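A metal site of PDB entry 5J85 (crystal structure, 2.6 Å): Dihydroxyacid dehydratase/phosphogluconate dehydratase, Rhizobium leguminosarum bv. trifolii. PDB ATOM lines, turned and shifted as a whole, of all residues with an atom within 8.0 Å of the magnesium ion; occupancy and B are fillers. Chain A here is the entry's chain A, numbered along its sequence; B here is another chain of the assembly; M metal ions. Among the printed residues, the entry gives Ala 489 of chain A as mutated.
The magnesium ion is bound by OE1 of Glu 462, OD2 of Asp 137, OE1 of Glu 100 and OQ1 of KCX 138.
Residues that only touch the magnesium ion: Thr 214. Five residues have an atom within 4 Å of the magnesium ion: Glu 100, Asp 137, KCX 138, Thr 214 and Glu 462. The nearest printed residue that does not touch the magnesium ion is Asn 287 (4.03 Å).
NH2 of Arg 487 is in salt-bridge range of OE2 of Glu 100. OG1 of Thr 106 sits at hydrogen-bond distance from OE2 of Glu 100, 3.3 Å away. SG of Cys 136 sits close to N of Glu 100, 3.5 Å away. OQ1 of KCX 138 lies close to the side-chain hydroxyl of Thr 214 (3.2 Å). OQ1 of KCX 138 lies close to the side-chain amide nitrogen of Asn 287. NH1 of Arg 487 lies within salt-bridge range of OQ2 of KCX 138 (3.3 Å). NE2 of His 291 lies within hydrogen-bond range of OQ2 of KCX 138 (2.7 Å). OG1 of Thr 214 is in hydrogen-bond range of OG of Ser 285, at 3.5 Å.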
ATOM      1  N   GLU A 100      29.432  15.640  23.737  1.00  0.00           N
ATOM      2  CA  GLU A 100      28.422  16.684  23.524  1.00  0.00           C
ATOM      3  C   GLU A 100      29.057  18.063  23.389  1.00  0.00           C
ATOM      4  O   GLU A 100      28.490  18.943  22.738  1.00  0.00           O
ATOM      5  CB  GLU A 100      27.395  16.677  24.657  1.00  0.00           C
ATOM      6  CG  GLU A 100      26.170  17.577  24.397  1.00  0.00           C
ATOM      7  CD  GLU A 100      24.892  16.835  23.971  1.00  0.00           C
ATOM      8  OE1 GLU A 100      24.235  16.250  24.874  1.00  0.00           O
ATOM      9  OE2 GLU A 100      24.527  16.857  22.760  1.00  0.00           O
ATOM     10  N   ASN A 101      30.229  18.271  23.979  1.00  0.00           N
ATOM     11  CA  ASN A 101      30.864  19.584  23.970  1.00  0.00           C
ATOM     12  C   ASN A 101      31.774  19.804  22.756  1.00  0.00           C
ATOM     13  O   ASN A 101      32.331  20.898  22.617  1.00  0.00           O
ATOM     14  CB  ASN A 101      31.646  19.809  25.265  1.00  0.00           C
ATOM     15  CG  ASN A 101      32.754  18.778  25.477  1.00  0.00           C
ATOM     16  OD1 ASN A 101      33.747  18.753  24.738  1.00  0.00           O
ATOM     17  ND2 ASN A 101      32.591  17.937  26.503  1.00  0.00           N
ATOM     18  N   THR A 106      25.024  17.801  16.758  1.00  0.00           N
ATOM     19  CA  THR A 106      24.736  17.447  18.144  1.00  0.00           C
ATOM     20  C   THR A 106      25.166  16.005  18.355  1.00  0.00           C
ATOM     21  O   THR A 106      24.952  15.158  17.482  1.00  0.00           O
ATOM     22  CB  THR A 106      23.245  17.624  18.514  1.00  0.00           C
ATOM     23  OG1 THR A 106      23.020  17.249  19.880  1.00  0.00           O
ATOM     24  CG2 THR A 106      22.326  16.801  17.606  1.00  0.00           C
ATOM     25  N   ALA A 107      25.770  15.736  19.519  1.00  0.00           N
ATOM     26  CA  ALA A 107      26.246  14.393  19.817  1.00  0.00           C
ATOM     27  C   ALA A 107      25.135  13.355  19.734  1.00  0.00           C
ATOM     28  O   ALA A 107      25.407  12.176  19.481  1.00  0.00           O
ATOM     29  CB  ALA A 107      26.904  14.368  21.196  1.00  0.00           C
ATOM     30  N   MET A 108      23.882  13.764  19.935  1.00  0.00           N
ATOM     31  CA  MET A 108      22.778  12.809  19.841  1.00  0.00           C
ATOM     32  C   MET A 108      22.729  12.134  18.474  1.00  0.00           C
ATOM     33  O   MET A 108      22.293  10.982  18.363  1.00  0.00           O
ATOM     34  CB  MET A 108      21.449  13.503  20.139  1.00  0.00           C
ATOM     35  CG  MET A 108      20.221  12.607  20.044  1.00  0.00           C
ATOM     36  SD  MET A 108      20.115  11.312  21.301  1.00  0.00           S
ATOM     37  CE  MET A 108      18.947  10.221  20.502  1.00  0.00           C
ATOM     38  N   CYS A 136      31.188  10.997  29.210  1.00  0.00           N
ATOM     39  CA  CYS A 136      30.450  12.111  28.614  1.00  0.00           C
ATOM     40  C   CYS A 136      29.089  11.650  28.099  1.00  0.00           C
ATOM     41  O   CYS A 136      28.929  10.533  27.605  1.00  0.00           O
ATOM     42  CB  CYS A 136      31.242  12.739  27.474  1.00  0.00           C
ATOM     43  SG  CYS A 136      30.440  14.213  26.729  1.00  0.00           S
ATOM     44  N   ASP A 137      28.123  12.563  28.210  1.00  0.00           N
ATOM     45  CA  ASP A 137      26.702  12.337  27.907  1.00  0.00           C
ATOM     46  C   ASP A 137      26.307  11.075  27.150  1.00  0.00           C
ATOM     47  O   ASP A 137      25.640  10.189  27.707  1.00  0.00           O
ATOM     48  CB  ASP A 137      26.169  13.544  27.127  1.00  0.00           C
ATOM     49  CG  ASP A 137      25.987  14.769  28.007  1.00  0.00           C
ATOM     50  OD1 ASP A 137      26.577  14.819  29.114  1.00  0.00           O
ATOM     51  OD2 ASP A 137      25.259  15.707  27.600  1.00  0.00           O
ATOM     52  N   KCX A 138      26.732  10.980  25.891  1.00  0.00           N
ATOM     53  CA  KCX A 138      26.207   9.941  24.986  1.00  0.00           C
ATOM     54  CB  KCX A 138      26.133  10.469  23.563  1.00  0.00           C
ATOM     55  CG  KCX A 138      25.249  11.692  23.507  1.00  0.00           C
ATOM     56  CD  KCX A 138      23.792  11.248  23.494  1.00  0.00           C
ATOM     57  CE  KCX A 138      22.875  12.461  23.448  1.00  0.00           C
ATOM     58  NZ  KCX A 138      23.343  13.405  24.406  1.00  0.00           N
ATOM     59  C   KCX A 138      27.029   8.675  24.990  1.00  0.00           C
ATOM     60  O   KCX A 138      26.648   7.723  24.313  1.00  0.00           O
ATOM     61  CX  KCX A 138      22.462  13.510  25.519  1.00  0.00           C
ATOM     62  OQ1 KCX A 138      22.683  14.375  26.414  1.00  0.00           O
ATOM     63  OQ2 KCX A 138      21.453  12.758  25.629  1.00  0.00           O
ATOM     64  N   CYS A 209      29.964  16.839  33.552  1.00  0.00           N
ATOM     65  CA  CYS A 209      29.207  17.933  34.152  1.00  0.00           C
ATOM     66  C   CYS A 209      28.744  17.555  35.557  1.00  0.00           C
ATOM     67  O   CYS A 209      28.110  16.520  35.751  1.00  0.00           O
ATOM     68  CB  CYS A 209      28.012  18.301  33.268  1.00  0.00           C
ATOM     69  SG  CYS A 209      28.449  18.742  31.561  1.00  0.00           S
ATOM     70  N   GLY A 213      22.936  16.595  35.293  1.00  0.00           N
ATOM     71  CA  GLY A 213      22.766  16.592  33.858  1.00  0.00           C
ATOM     72  C   GLY A 213      22.753  15.181  33.304  1.00  0.00           C
ATOM     73  O   GLY A 213      22.656  14.188  34.027  1.00  0.00           O
ATOM     74  N   THR A 214      22.893  15.095  31.971  1.00  0.00           N
ATOM     75  CA  THR A 214      22.754  13.808  31.304  1.00  0.00           C
ATOM     76  C   THR A 214      23.831  12.817  31.734  1.00  0.00           C
ATOM     77  O   THR A 214      23.572  11.617  31.831  1.00  0.00           O
ATOM     78  CB  THR A 214      22.763  13.981  29.797  1.00  0.00           C
ATOM     79  OG1 THR A 214      21.857  15.029  29.427  1.00  0.00           O
ATOM     80  CG2 THR A 214      22.370  12.689  29.110  1.00  0.00           C
ATOM     81  N   ALA A 215      25.054  13.308  31.982  1.00  0.00           N
ATOM     82  CA  ALA A 215      26.138  12.406  32.365  1.00  0.00           C
ATOM     83  C   ALA A 215      25.905  11.814  33.753  1.00  0.00           C
ATOM     84  O   ALA A 215      26.000  10.590  33.932  1.00  0.00           O
ATOM     85  CB  ALA A 215      27.481  13.144  32.315  1.00  0.00           C
ATOM     86  N   SER A 285      17.872  13.826  34.201  1.00  0.00           N
ATOM     87  CA  SER A 285      17.645  14.437  32.903  1.00  0.00           C
ATOM     88  C   SER A 285      16.513  13.741  32.155  1.00  0.00           C
ATOM     89  O   SER A 285      16.363  12.521  32.209  1.00  0.00           O
ATOM     90  CB  SER A 285      18.948  14.391  32.083  1.00  0.00           C
ATOM     91  OG  SER A 285      18.678  14.619  30.705  1.00  0.00           O
ATOM     92  N   ASN A 287      16.734  13.291  29.240  1.00  0.00           N
ATOM     93  CA  ASN A 287      17.414  12.500  28.217  1.00  0.00           C
ATOM     94  C   ASN A 287      17.409  11.017  28.554  1.00  0.00           C
ATOM     95  O   ASN A 287      17.427  10.178  27.648  1.00  0.00           O
ATOM     96  CB  ASN A 287      18.847  13.001  28.043  1.00  0.00           C
ATOM     97  CG  ASN A 287      18.901  14.331  27.344  1.00  0.00           C
ATOM     98  OD1 ASN A 287      18.193  14.549  26.357  1.00  0.00           O
ATOM     99  ND2 ASN A 287      19.725  15.233  27.864  1.00  0.00           N
ATOM    100  N   HIS A 291      17.224   7.439  26.198  1.00  0.00           N
ATOM    101  CA  HIS A 291      18.298   6.452  26.193  1.00  0.00           C
ATOM    102  C   HIS A 291      17.831   5.103  26.743  1.00  0.00           C
ATOM    103  O   HIS A 291      18.139   4.060  26.156  1.00  0.00           O
ATOM    104  CB  HIS A 291      19.482   6.997  26.979  1.00  0.00           C
ATOM    105  CG  HIS A 291      20.122   8.177  26.326  1.00  0.00           C
ATOM    106  ND1 HIS A 291      20.242   8.282  24.953  1.00  0.00           N
ATOM    107  CD2 HIS A 291      20.668   9.305  26.843  1.00  0.00           C
ATOM    108  CE1 HIS A 291      20.841   9.419  24.650  1.00  0.00           C
ATOM    109  NE2 HIS A 291      21.114  10.056  25.781  1.00  0.00           N
ATOM    110  N   GLU A 462      19.637  19.921  21.850  1.00  0.00           N
ATOM    111  CA  GLU A 462      19.150  20.415  23.147  1.00  0.00           C
ATOM    112  C   GLU A 462      18.763  21.896  23.036  1.00  0.00           C
ATOM    113  O   GLU A 462      19.355  22.779  23.660  1.00  0.00           O
ATOM    114  CB  GLU A 462      20.203  20.195  24.223  1.00  0.00           C
ATOM    115  CG  GLU A 462      20.413  18.728  24.582  1.00  0.00           C
ATOM    116  CD  GLU A 462      21.539  18.518  25.576  1.00  0.00           C
ATOM    117  OE1 GLU A 462      21.773  17.346  25.960  1.00  0.00           O
ATOM    118  OE2 GLU A 462      22.200  19.499  25.969  1.00  0.00           O
ATOM    119  N   ARG A 487      15.180  18.103  22.277  1.00  0.00           N
ATOM    120  CA  ARG A 487      15.596  17.656  23.584  1.00  0.00           C
ATOM    121  C   ARG A 487      15.900  18.865  24.456  1.00  0.00           C
ATOM    122  O   ARG A 487      15.759  20.015  24.048  1.00  0.00           O
ATOM    123  CB  ARG A 487      16.811  16.735  23.513  1.00  0.00           C
ATOM    124  CG  ARG A 487      16.507  15.300  23.198  1.00  0.00           C
ATOM    125  CD  ARG A 487      17.756  14.434  23.191  1.00  0.00           C
ATOM    126  NE  ARG A 487      18.840  15.028  22.410  1.00  0.00           N
ATOM    127  CZ  ARG A 487      19.970  15.499  22.930  1.00  0.00           C
ATOM    128  NH1 ARG A 487      20.182  15.433  24.241  1.00  0.00           N
ATOM    129  NH2 ARG A 487      20.898  16.026  22.140  1.00  0.00           N
ATOM    130  N   MET A 488      16.388  18.598  25.642  1.00  0.00           N
ATOM    131  CA  MET A 488      16.715  19.616  26.619  1.00  0.00           C
ATOM    132  C   MET A 488      17.908  19.091  27.392  1.00  0.00           C
ATOM    133  O   MET A 488      17.998  17.889  27.642  1.00  0.00           O
ATOM    134  CB  MET A 488      15.514  19.850  27.522  1.00  0.00           C
ATOM    135  CG  MET A 488      15.780  20.672  28.736  1.00  0.00           C
ATOM    136  SD  MET A 488      14.233  21.311  29.346  1.00  0.00           S
ATOM    137  CE  MET A 488      14.012  20.335  30.839  1.00  0.00           C
ATOM    138  N   ALA A 489      18.830  19.979  27.731  1.00  0.00           N
ATOM    139  CA  ALA A 489      19.920  19.562  28.607  1.00  0.00           C
ATOM    140  C   ALA A 489      19.344  19.053  29.937  1.00  0.00           C
ATOM    141  O   ALA A 489      18.271  19.466  30.369  1.00  0.00           O
ATOM    142  CB  ALA A 489      20.876  20.723  28.859  1.00  0.00           C
ATOM    143  N   GLY A 490      20.077  18.131  30.566  1.00  0.00           N
ATOM    144  CA  GLY A 490      19.744  17.782  31.939  1.00  0.00           C
ATOM    145  C   GLY A 490      19.657  19.009  32.824  1.00  0.00           C
ATOM    146  O   GLY A 490      18.819  19.058  33.742  1.00  0.00           O
ATOM    147  N   THR A 491      20.487  20.007  32.570  1.00  0.00           N
ATOM    148  CA  THR A 491      20.440  21.299  33.255  1.00  0.00           C
ATOM    149  C   THR A 491      19.370  22.159  32.594  1.00  0.00           C
ATOM    150  O   THR A 491      19.538  22.588  31.443  1.00  0.00           O
ATOM    151  CB  THR A 491      21.809  21.982  33.192  1.00  0.00           C
ATOM    152  OG1 THR A 491      22.862  20.996  33.305  1.00  0.00           O
ATOM    153  CG2 THR A 491      21.979  23.042  34.307  1.00  0.00           C
ATOM    154  N   TYR B  35      31.462  27.455  26.505  1.00  0.00           N
ATOM    155  CA  TYR B  35      31.126  26.051  26.722  1.00  0.00           C
ATOM    156  C   TYR B  35      32.207  25.158  26.114  1.00  0.00           C
ATOM    157  O   TYR B  35      32.868  24.389  26.823  1.00  0.00           O
ATOM    158  CB  TYR B  35      29.758  25.748  26.111  1.00  0.00           C
ATOM    159  CG  TYR B  35      29.329  24.281  26.156  1.00  0.00           C
ATOM    160  CD1 TYR B  35      29.269  23.580  27.364  1.00  0.00           C
ATOM    161  CD2 TYR B  35      28.976  23.605  24.985  1.00  0.00           C
ATOM    162  CE1 TYR B  35      28.874  22.240  27.403  1.00  0.00           C
ATOM    163  CE2 TYR B  35      28.577  22.270  25.017  1.00  0.00           C
ATOM    164  CZ  TYR B  35      28.529  21.600  26.226  1.00  0.00           C
ATOM    165  OH  TYR B  35      28.139  20.284  26.267  1.00  0.00           O
ATOM    166  N   SER B 587      25.119  22.881  18.571  1.00  0.00           N
ATOM    167  CA  SER B 587      24.339  21.920  19.333  1.00  0.00           C
ATOM    168  C   SER B 587      23.481  22.553  20.414  1.00  0.00           C
ATOM    169  O   SER B 587      22.712  21.833  21.077  1.00  0.00           O
ATOM    170  CB  SER B 587      25.263  20.854  19.948  1.00  0.00           C
ATOM    171  OG  SER B 587      26.378  21.439  20.598  1.00  0.00           O
HETATM  172 MG    MG M   1      23.419  16.610  27.030  1.00  0.00          MG
